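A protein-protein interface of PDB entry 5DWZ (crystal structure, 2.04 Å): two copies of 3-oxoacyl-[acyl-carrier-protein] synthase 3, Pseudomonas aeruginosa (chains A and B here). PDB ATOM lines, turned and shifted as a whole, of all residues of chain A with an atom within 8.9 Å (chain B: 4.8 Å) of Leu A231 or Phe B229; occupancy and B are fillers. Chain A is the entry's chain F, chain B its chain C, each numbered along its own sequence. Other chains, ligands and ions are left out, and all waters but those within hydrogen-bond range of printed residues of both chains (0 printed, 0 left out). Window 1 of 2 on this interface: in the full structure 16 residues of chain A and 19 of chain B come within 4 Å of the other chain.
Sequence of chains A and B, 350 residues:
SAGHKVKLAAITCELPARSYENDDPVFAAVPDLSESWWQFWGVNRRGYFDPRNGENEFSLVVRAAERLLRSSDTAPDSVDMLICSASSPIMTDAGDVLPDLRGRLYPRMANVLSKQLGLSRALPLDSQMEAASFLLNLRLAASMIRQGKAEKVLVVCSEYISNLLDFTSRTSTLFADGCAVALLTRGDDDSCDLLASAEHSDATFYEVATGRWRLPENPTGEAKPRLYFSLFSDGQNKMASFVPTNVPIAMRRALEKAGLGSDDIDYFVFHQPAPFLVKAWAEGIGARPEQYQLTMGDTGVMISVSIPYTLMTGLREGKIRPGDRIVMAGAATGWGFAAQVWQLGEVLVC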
ATOM      1  N   THR A 204      14.566   7.850   1.604  1.00  0.00           N
ATOM      2  CA  THR A 204      15.341   6.633   1.151  1.00  0.00           C
ATOM      3  C   THR A 204      15.147   5.464   2.103  1.00  0.00           C
ATOM      4  O   THR A 204      14.927   4.370   1.678  1.00  0.00           O
ATOM      5  CB  THR A 204      16.866   6.944   1.032  1.00  0.00           C
ATOM      6  OG1 THR A 204      17.062   7.981   0.055  1.00  0.00           O
ATOM      7  CG2 THR A 204      17.667   5.731   0.611  1.00  0.00           C
ATOM      8  N   PHE A 205      15.290   5.761   3.381  1.00  0.00           N
ATOM      9  CA  PHE A 205      15.196   4.818   4.462  1.00  0.00           C
ATOM     10  C   PHE A 205      13.924   4.929   5.282  1.00  0.00           C
ATOM     11  O   PHE A 205      13.894   4.537   6.436  1.00  0.00           O
ATOM     12  CB  PHE A 205      16.437   4.917   5.387  1.00  0.00           C
ATOM     13  CG  PHE A 205      17.714   4.538   4.702  1.00  0.00           C
ATOM     14  CD1 PHE A 205      17.920   3.213   4.263  1.00  0.00           C
ATOM     15  CD2 PHE A 205      18.696   5.491   4.415  1.00  0.00           C
ATOM     16  CE1 PHE A 205      19.097   2.869   3.584  1.00  0.00           C
ATOM     17  CE2 PHE A 205      19.865   5.143   3.746  1.00  0.00           C
ATOM     18  CZ  PHE A 205      20.061   3.831   3.326  1.00  0.00           C
ATOM     19  N   TYR A 206      12.877   5.399   4.631  1.00  0.00           N
ATOM     20  CA  TYR A 206      11.537   5.525   5.249  1.00  0.00           C
ATOM     21  C   TYR A 206      11.152   4.242   6.005  1.00  0.00           C
ATOM     22  O   TYR A 206      10.728   4.289   7.138  1.00  0.00           O
ATOM     23  CB  TYR A 206      10.476   5.827   4.171  1.00  0.00           C
ATOM     24  CG  TYR A 206       9.099   5.618   4.707  1.00  0.00           C
ATOM     25  CD1 TYR A 206       8.605   6.471   5.710  1.00  0.00           C
ATOM     26  CD2 TYR A 206       8.286   4.547   4.280  1.00  0.00           C
ATOM     27  CE1 TYR A 206       7.348   6.266   6.297  1.00  0.00           C
ATOM     28  CE2 TYR A 206       7.022   4.342   4.841  1.00  0.00           C
ATOM     29  CZ  TYR A 206       6.552   5.218   5.851  1.00  0.00           C
ATOM     30  OH  TYR A 206       5.320   5.068   6.443  1.00  0.00           O
ATOM     31  N   GLU A 207      11.317   3.102   5.341  1.00  0.00           N
ATOM     32  CA  GLU A 207      10.795   1.804   5.849  1.00  0.00           C
ATOM     33  C   GLU A 207      11.606   1.184   6.956  1.00  0.00           C
ATOM     34  O   GLU A 207      11.172   0.222   7.578  1.00  0.00           O
ATOM     35  CB  GLU A 207      10.656   0.791   4.722  1.00  0.00           C
ATOM     36  CG  GLU A 207       9.730   1.286   3.635  1.00  0.00           C
ATOM     37  CD  GLU A 207       9.581   0.331   2.474  1.00  0.00           C
ATOM     38  OE1 GLU A 207       9.478  -0.900   2.698  1.00  0.00           O
ATOM     39  OE2 GLU A 207       9.536   0.841   1.331  1.00  0.00           O
ATOM     40  N   VAL A 208      12.745   1.783   7.247  1.00  0.00           N
ATOM     41  CA  VAL A 208      13.626   1.313   8.331  1.00  0.00           C
ATOM     42  C   VAL A 208      12.995   1.331   9.719  1.00  0.00           C
ATOM     43  O   VAL A 208      13.290   0.508  10.547  1.00  0.00           O
ATOM     44  CB  VAL A 208      14.943   2.123   8.358  1.00  0.00           C
ATOM     45  CG1 VAL A 208      15.752   1.894   9.630  1.00  0.00           C
ATOM     46  CG2 VAL A 208      15.777   1.734   7.148  1.00  0.00           C
ATOM     47  N   ALA A 209      12.120   2.298   9.967  1.00  0.00           N
ATOM     48  CA  ALA A 209      11.515   2.472  11.285  1.00  0.00           C
ATOM     49  C   ALA A 209      10.106   2.935  11.063  1.00  0.00           C
ATOM     50  O   ALA A 209       9.862   4.093  10.682  1.00  0.00           O
ATOM     51  CB  ALA A 209      12.297   3.461  12.141  1.00  0.00           C
ATOM     52  N   ARG A 212       3.530  -0.063  13.195  1.00  0.00           N
ATOM     53  CA  ARG A 212       2.534  -0.987  12.613  1.00  0.00           C
ATOM     54  C   ARG A 212       1.622  -1.562  13.641  1.00  0.00           C
ATOM     55  O   ARG A 212       2.018  -1.807  14.775  1.00  0.00           O
ATOM     56  CB  ARG A 212       3.204  -2.125  11.855  1.00  0.00           C
ATOM     57  CG  ARG A 212       4.335  -1.640  10.965  1.00  0.00           C
ATOM     58  CD  ARG A 212       4.895  -2.765  10.090  1.00  0.00           C
ATOM     59  NE  ARG A 212       6.143  -2.354   9.461  1.00  0.00           N
ATOM     60  CZ  ARG A 212       6.848  -3.092   8.606  1.00  0.00           C
ATOM     61  NH1 ARG A 212       6.438  -4.307   8.267  1.00  0.00           N
ATOM     62  NH2 ARG A 212       7.983  -2.618   8.092  1.00  0.00           N
ATOM     63  N   TYR A 228       8.521  -1.392  14.184  1.00  0.00           N
ATOM     64  CA  TYR A 228       9.053  -2.410  13.271  1.00  0.00           C
ATOM     65  C   TYR A 228      10.288  -1.851  12.585  1.00  0.00           C
ATOM     66  O   TYR A 228      10.287  -0.702  12.129  1.00  0.00           O
ATOM     67  CB  TYR A 228       8.054  -2.820  12.208  1.00  0.00           C
ATOM     68  CG  TYR A 228       7.054  -3.838  12.703  1.00  0.00           C
ATOM     69  CD1 TYR A 228       6.076  -3.486  13.647  1.00  0.00           C
ATOM     70  CD2 TYR A 228       7.071  -5.148  12.239  1.00  0.00           C
ATOM     71  CE1 TYR A 228       5.150  -4.407  14.122  1.00  0.00           C
ATOM     72  CE2 TYR A 228       6.143  -6.082  12.705  1.00  0.00           C
ATOM     73  CZ  TYR A 228       5.182  -5.702  13.646  1.00  0.00           C
ATOM     74  OH  TYR A 228       4.268  -6.609  14.107  1.00  0.00           O
ATOM     75  N   PHE A 229      11.337  -2.674  12.564  1.00  0.00           N
ATOM     76  CA  PHE A 229      12.559  -2.400  11.786  1.00  0.00           C
ATOM     77  C   PHE A 229      12.579  -3.172  10.493  1.00  0.00           C
ATOM     78  O   PHE A 229      12.194  -4.335  10.460  1.00  0.00           O
ATOM     79  CB  PHE A 229      13.809  -2.707  12.587  1.00  0.00           C
ATOM     80  CG  PHE A 229      13.903  -1.896  13.832  1.00  0.00           C
ATOM     81  CD1 PHE A 229      14.140  -0.528  13.765  1.00  0.00           C
ATOM     82  CD2 PHE A 229      13.730  -2.486  15.070  1.00  0.00           C
ATOM     83  CE1 PHE A 229      14.207   0.251  14.915  1.00  0.00           C
ATOM     84  CE2 PHE A 229      13.792  -1.717  16.230  1.00  0.00           C
ATOM     85  CZ  PHE A 229      14.036  -0.349  16.154  1.00  0.00           C
ATOM     86  N   SER A 230      13.054  -2.522   9.438  1.00  0.00           N
ATOM     87  CA  SER A 230      13.126  -3.134   8.101  1.00  0.00           C
ATOM     88  C   SER A 230      14.194  -2.547   7.113  1.00  0.00           C
ATOM     89  O   SER A 230      13.904  -1.753   6.197  1.00  0.00           O
ATOM     90  CB  SER A 230      11.766  -3.029   7.510  1.00  0.00           C
ATOM     91  OG  SER A 230      11.695  -3.770   6.338  1.00  0.00           O
ATOM     92  N   LEU A 231      15.444  -2.961   7.323  1.00  0.00           N
ATOM     93  CA  LEU A 231      16.586  -2.589   6.441  1.00  0.00           C
ATOM     94  C   LEU A 231      16.891  -3.770   5.528  1.00  0.00           C
ATOM     95  O   LEU A 231      17.163  -4.858   6.005  1.00  0.00           O
ATOM     96  CB  LEU A 231      17.865  -2.156   7.211  1.00  0.00           C
ATOM     97  CG  LEU A 231      18.844  -1.158   6.581  1.00  0.00           C
ATOM     98  CD1 LEU A 231      20.288  -1.256   7.087  1.00  0.00           C
ATOM     99  CD2 LEU A 231      18.822  -1.179   5.059  1.00  0.00           C
ATOM    100  N   PHE A 232      16.806  -3.531   4.224  1.00  0.00           N
ATOM    101  CA  PHE A 232      17.196  -4.482   3.193  1.00  0.00           C
ATOM    102  C   PHE A 232      18.123  -3.679   2.301  1.00  0.00           C
ATOM    103  O   PHE A 232      17.617  -2.865   1.556  1.00  0.00           O
ATOM    104  CB  PHE A 232      15.987  -5.050   2.403  1.00  0.00           C
ATOM    105  CG  PHE A 232      14.749  -4.217   2.485  1.00  0.00           C
ATOM    106  CD1 PHE A 232      13.869  -4.404   3.516  1.00  0.00           C
ATOM    107  CE1 PHE A 232      12.724  -3.649   3.597  1.00  0.00           C
ATOM    108  CZ  PHE A 232      12.449  -2.701   2.627  1.00  0.00           C
ATOM    109  N   SER A 233      19.450  -3.843   2.427  1.00  0.00           N
ATOM    110  CA  SER A 233      20.378  -3.162   1.523  1.00  0.00           C
ATOM    111  C   SER A 233      21.672  -3.830   1.120  1.00  0.00           C
ATOM    112  O   SER A 233      22.350  -4.520   1.868  1.00  0.00           O
ATOM    113  CB  SER A 233      20.733  -1.745   1.998  1.00  0.00           C
ATOM    114  OG  SER A 233      22.063  -1.682   2.524  1.00  0.00           O
ATOM    115  N   ASP A 234      21.981  -3.422  -0.097  1.00  0.00           N
ATOM    116  CA  ASP A 234      23.114  -3.728  -0.949  1.00  0.00           C
ATOM    117  C   ASP A 234      24.355  -2.920  -0.604  1.00  0.00           C
ATOM    118  O   ASP A 234      25.459  -3.312  -0.979  1.00  0.00           O
ATOM    119  CB  ASP A 234      22.666  -3.296  -2.413  1.00  0.00           C
ATOM    120  CG  ASP A 234      23.208  -4.171  -3.463  1.00  0.00           C
ATOM    121  OD1 ASP A 234      24.216  -4.835  -3.210  1.00  0.00           O
ATOM    122  OD2 ASP A 234      22.643  -4.209  -4.576  1.00  0.00           O
ATOM    123  N   GLY A 235      24.150  -1.776   0.058  1.00  0.00           N
ATOM    124  CA  GLY A 235      25.156  -0.716   0.191  1.00  0.00           C
ATOM    125  C   GLY A 235      25.070   0.306  -0.949  1.00  0.00           C
ATOM    126  O   GLY A 235      25.593   1.394  -0.816  1.00  0.00           O
ATOM    127  N   GLN A 236      24.424  -0.041  -2.066  1.00  0.00           N
ATOM    128  CA  GLN A 236      24.432   0.780  -3.288  1.00  0.00           C
ATOM    129  C   GLN A 236      23.397   1.873  -3.342  1.00  0.00           C
ATOM    130  O   GLN A 236      23.523   2.777  -4.161  1.00  0.00           O
ATOM    131  CB  GLN A 236      24.267  -0.089  -4.535  1.00  0.00           C
ATOM    132  CG  GLN A 236      25.245  -1.250  -4.627  1.00  0.00           C
ATOM    133  CD  GLN A 236      25.181  -1.947  -5.991  1.00  0.00           C
ATOM    134  OE1 GLN A 236      24.673  -3.065  -6.094  1.00  0.00           O
ATOM    135  NE2 GLN A 236      25.711  -1.300  -7.037  1.00  0.00           N
ATOM    136  N   ASN A 237      22.371   1.775  -2.505  1.00  0.00           N
ATOM    137  CA  ASN A 237      21.307   2.782  -2.457  1.00  0.00           C
ATOM    138  C   ASN A 237      21.356   3.645  -1.190  1.00  0.00           C
ATOM    139  O   ASN A 237      20.627   3.430  -0.224  1.00  0.00           O
ATOM    140  CB  ASN A 237      19.930   2.170  -2.709  1.00  0.00           C
ATOM    141  CG  ASN A 237      18.865   3.236  -2.971  1.00  0.00           C
ATOM    142  OD1 ASN A 237      19.199   4.357  -3.345  1.00  0.00           O
ATOM    143  ND2 ASN A 237      17.588   2.912  -2.740  1.00  0.00           N
ATOM    144  N   THR B 171      31.720  -0.722   4.718  1.00  0.00           N
ATOM    145  CA  THR B 171      32.108  -2.120   5.028  1.00  0.00           C
ATOM    146  C   THR B 171      33.523  -2.446   4.583  1.00  0.00           C
ATOM    147  O   THR B 171      34.188  -3.268   5.224  1.00  0.00           O
ATOM    148  CB  THR B 171      31.141  -3.182   4.444  1.00  0.00           C
ATOM    149  OG1 THR B 171      30.909  -2.899   3.074  1.00  0.00           O
ATOM    150  CG2 THR B 171      29.862  -3.185   5.176  1.00  0.00           C
ATOM    151  N   VAL B 208      20.575 -12.331   7.836  1.00  0.00           N
ATOM    152  CA  VAL B 208      21.072 -11.002   8.185  1.00  0.00           C
ATOM    153  C   VAL B 208      22.264 -10.518   7.357  1.00  0.00           C
ATOM    154  O   VAL B 208      22.400  -9.347   7.083  1.00  0.00           O
ATOM    155  CB  VAL B 208      21.414 -10.931   9.701  1.00  0.00           C
ATOM    156  CG1 VAL B 208      22.235  -9.711  10.058  1.00  0.00           C
ATOM    157  CG2 VAL B 208      20.118 -10.918  10.458  1.00  0.00           C
ATOM    158  N   ALA B 209      23.132 -11.433   7.009  1.00  0.00           N
ATOM    159  CA  ALA B 209      24.368 -11.137   6.292  1.00  0.00           C
ATOM    160  C   ALA B 209      24.569 -12.264   5.305  1.00  0.00           C
ATOM    161  O   ALA B 209      24.895 -13.408   5.667  1.00  0.00           O
ATOM    162  CB  ALA B 209      25.570 -11.040   7.242  1.00  0.00           C
ATOM    163  N   LEU B 227      27.904  -8.216  -0.237  1.00  0.00           N
ATOM    164  CA  LEU B 227      27.277  -8.320   1.054  1.00  0.00           C
ATOM    165  C   LEU B 227      25.953  -7.633   0.990  1.00  0.00           C
ATOM    166  O   LEU B 227      25.829  -6.545   0.519  1.00  0.00           O
ATOM    167  CB  LEU B 227      28.065  -7.587   2.104  1.00  0.00           C
ATOM    168  CG  LEU B 227      28.860  -8.303   3.146  1.00  0.00           C
ATOM    169  CD1 LEU B 227      29.868  -7.390   3.808  1.00  0.00           C
ATOM    170  CD2 LEU B 227      27.966  -8.965   4.159  1.00  0.00           C
ATOM    171  N   TYR B 228      24.972  -8.303   1.504  1.00  0.00           N
ATOM    172  CA  TYR B 228      23.603  -7.819   1.571  1.00  0.00           C
ATOM    173  C   TYR B 228      23.129  -8.009   3.009  1.00  0.00           C
ATOM    174  O   TYR B 228      23.400  -9.041   3.650  1.00  0.00           O
ATOM    175  CB  TYR B 228      22.764  -8.576   0.550  1.00  0.00           C
ATOM    176  CG  TYR B 228      21.427  -7.997   0.241  1.00  0.00           C
ATOM    177  CD1 TYR B 228      20.377  -8.126   1.147  1.00  0.00           C
ATOM    178  CD2 TYR B 228      21.176  -7.354  -0.954  1.00  0.00           C
ATOM    179  CE1 TYR B 228      19.104  -7.632   0.883  1.00  0.00           C
ATOM    180  CE2 TYR B 228      19.908  -6.851  -1.227  1.00  0.00           C
ATOM    181  CZ  TYR B 228      18.884  -6.986  -0.298  1.00  0.00           C
ATOM    182  OH  TYR B 228      17.658  -6.454  -0.547  1.00  0.00           O
ATOM    183  N   PHE B 229      22.540  -6.941   3.549  1.00  0.00           N
ATOM    184  CA  PHE B 229      21.965  -6.931   4.909  1.00  0.00           C
ATOM    185  C   PHE B 229      20.461  -6.978   4.834  1.00  0.00           C
ATOM    186  O   PHE B 229      19.883  -6.319   3.993  1.00  0.00           O
ATOM    187  CB  PHE B 229      22.437  -5.741   5.719  1.00  0.00           C
ATOM    188  CG  PHE B 229      23.913  -5.702   5.837  1.00  0.00           C
ATOM    189  CD1 PHE B 229      24.575  -6.638   6.612  1.00  0.00           C
ATOM    190  CD2 PHE B 229      24.654  -4.792   5.092  1.00  0.00           C
ATOM    191  CE1 PHE B 229      25.967  -6.654   6.667  1.00  0.00           C
ATOM    192  CE2 PHE B 229      26.041  -4.781   5.157  1.00  0.00           C
ATOM    193  CZ  PHE B 229      26.700  -5.715   5.950  1.00  0.00           C
ATOM    194  N   SER B 230      19.866  -7.822   5.674  1.00  0.00           N
ATOM    195  CA  SER B 230      18.397  -8.000   5.745  1.00  0.00           C
ATOM    196  C   SER B 230      18.059  -8.137   7.212  1.00  0.00           C
ATOM    197  O   SER B 230      18.393  -9.144   7.799  1.00  0.00           O
ATOM    198  CB  SER B 230      17.872  -9.273   5.046  1.00  0.00           C
ATOM    199  OG  SER B 230      17.328  -9.036   3.788  1.00  0.00           O
ATOM    200  N   LEU B 231      17.426  -7.133   7.798  1.00  0.00           N
ATOM    201  CA  LEU B 231      16.784  -7.280   9.115  1.00  0.00           C
ATOM    202  C   LEU B 231      15.356  -6.775   9.102  1.00  0.00           C
ATOM    203  O   LEU B 231      15.085  -5.681   8.608  1.00  0.00           O
ATOM    204  CB  LEU B 231      17.534  -6.595  10.235  1.00  0.00           C
ATOM    205  CG  LEU B 231      18.878  -5.971   9.878  1.00  0.00           C
ATOM    206  CD1 LEU B 231      18.703  -4.609   9.222  1.00  0.00           C
ATOM    207  CD2 LEU B 231      19.809  -5.869  11.084  1.00  0.00           C
ATOM    208  N   PHE B 232      14.464  -7.604   9.634  1.00  0.00           N
ATOM    209  CA  PHE B 232      13.035  -7.351   9.682  1.00  0.00           C
ATOM    210  C   PHE B 232      12.574  -7.698  11.094  1.00  0.00           C
ATOM    211  O   PHE B 232      13.027  -8.667  11.637  1.00  0.00           O
ATOM    212  CB  PHE B 232      12.301  -8.223   8.668  1.00  0.00           C
ATOM    213  CG  PHE B 232      12.692  -8.001   7.222  1.00  0.00           C
ATOM    214  CD1 PHE B 232      13.538  -6.961   6.810  1.00  0.00           C
ATOM    215  CD2 PHE B 232      12.144  -8.812   6.240  1.00  0.00           C
ATOM    216  CE1 PHE B 232      13.871  -6.780   5.474  1.00  0.00           C
ATOM    217  CE2 PHE B 232      12.473  -8.632   4.904  1.00  0.00           C
ATOM    218  CZ  PHE B 232      13.341  -7.622   4.518  1.00  0.00           C
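N of Phe B229 sits at hydrogen-bond distance from O of Ser A233 (3.0 Å).
O of Leu A231 lies within hydrogen-bond range of N of Leu B231, at 2.9 Å.
The backbone carbonyl oxygen (O) of Val B208 is in hydrogen-bond range of the backbone NH (N) of Ser B230 (3.3 Å).
The backbone carbonyl oxygen (O) of Val A208 sits at hydrogen-bond distance from the backbone NH (N) of Ser A230, at 3.2 Å.
The side-chain hydroxyl (OG) of Ser A233 lies within hydrogen-bond range of the backbone NH (N) of Gly A235.
The side-chain amide oxygen of Gln A236 lies close to the side-chain carboxylate of Asp A234.
Among the printed residues, merely in contact across the chains: Phe A229 with Leu B231 (3.7 Å), Phe A229 with Phe B232 (3.2 Å), Ser A230 with Leu B231 (3.3 Å), Ser A230 with Phe B232 (3.7 Å), Leu A231 with Phe B229 (3.7 Å), Leu A231 with Ser B230 (3.4 Å), Leu A231 with Phe B232 (3.8 Å), Phe A232 with Tyr B228 (3.7 Å), Phe A232 with Phe B229 (3.4 Å), Phe A232 with Phe B232 (3.1 Å), Ser A233 with Tyr B228 (3.5 Å) and Asp A234 with Leu B227 (3.6 Å).
Thr A204 touches none of the printed residues of chain B.
Of the printed residues of chain B, Phe A229 touches Leu B231 (3.7 Å) and Phe B232 (3.2 Å).
Leu A231 touches four residues of chain B.
Ala B209 touches none of the printed residues of chain A.
Of the printed residues of chain A, Leu B227 touches Asp A234 (3.6 Å).
Printed residues of chain A within 4 Å of Tyr B228: Phe A232 and Ser A233.
Phe B229 touches just these residues of chain A: Leu A231, Phe A232 and Ser A233.
Of chain A, only Leu A231 (3.4 Å) comes within 4 Å of Ser B230.
Of the printed residues of chain A, Phe B232 touches Phe A229, Ser A230, Leu A231 and Phe A232.
The nearest residue of chain A that does not touch Phe B229 is Asp A234 (5.1 Å).
The nearest printed residue of chain A that does not touch Tyr B228 is Asp A234 (4.1 Å).
Printed residues of chain A that touch a printed residue of chain B: Phe A229, Ser A230, Leu A231, Phe A232, Ser A233 and Asp A234.
Hydrophobic or aromatic side chains of chain A that line the printed part of chain B: Leu A231 and Phe A232.
Of the 9 printed residues of chain B, 6 touch a printed residue of chain A.
Printed residues of chain B that touch a printed residue of chain A: Leu B227, Tyr B228, Phe B229, Ser B230, Leu B231 and Phe B232.
Hydrophobic or aromatic side chains of chain B within 4 Å of the printed part of chain A: Tyr B228, Phe B229, Leu B231 and Phe B232.
Among the printed residues, 14 pairs touch across the chains.
Phe A229 touches Phe B232, and with the chains exchanged Phe A232 touches Phe B229.
Ser A230 touches Phe B232, but with the chains exchanged Phe A232 does not touch Ser B230 (4.4 Å).
Leu A231 touches Phe B232, but with the chains exchanged Phe A232 does not touch Leu B231 (5.1 Å).
Phe A232 touches Tyr B228, but with the chains exchanged Tyr A228 does not touch Phe B232 (6.2 Å).
Positions printed for both chains: 208, 209, 228, 229, 230, 231 and 232.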
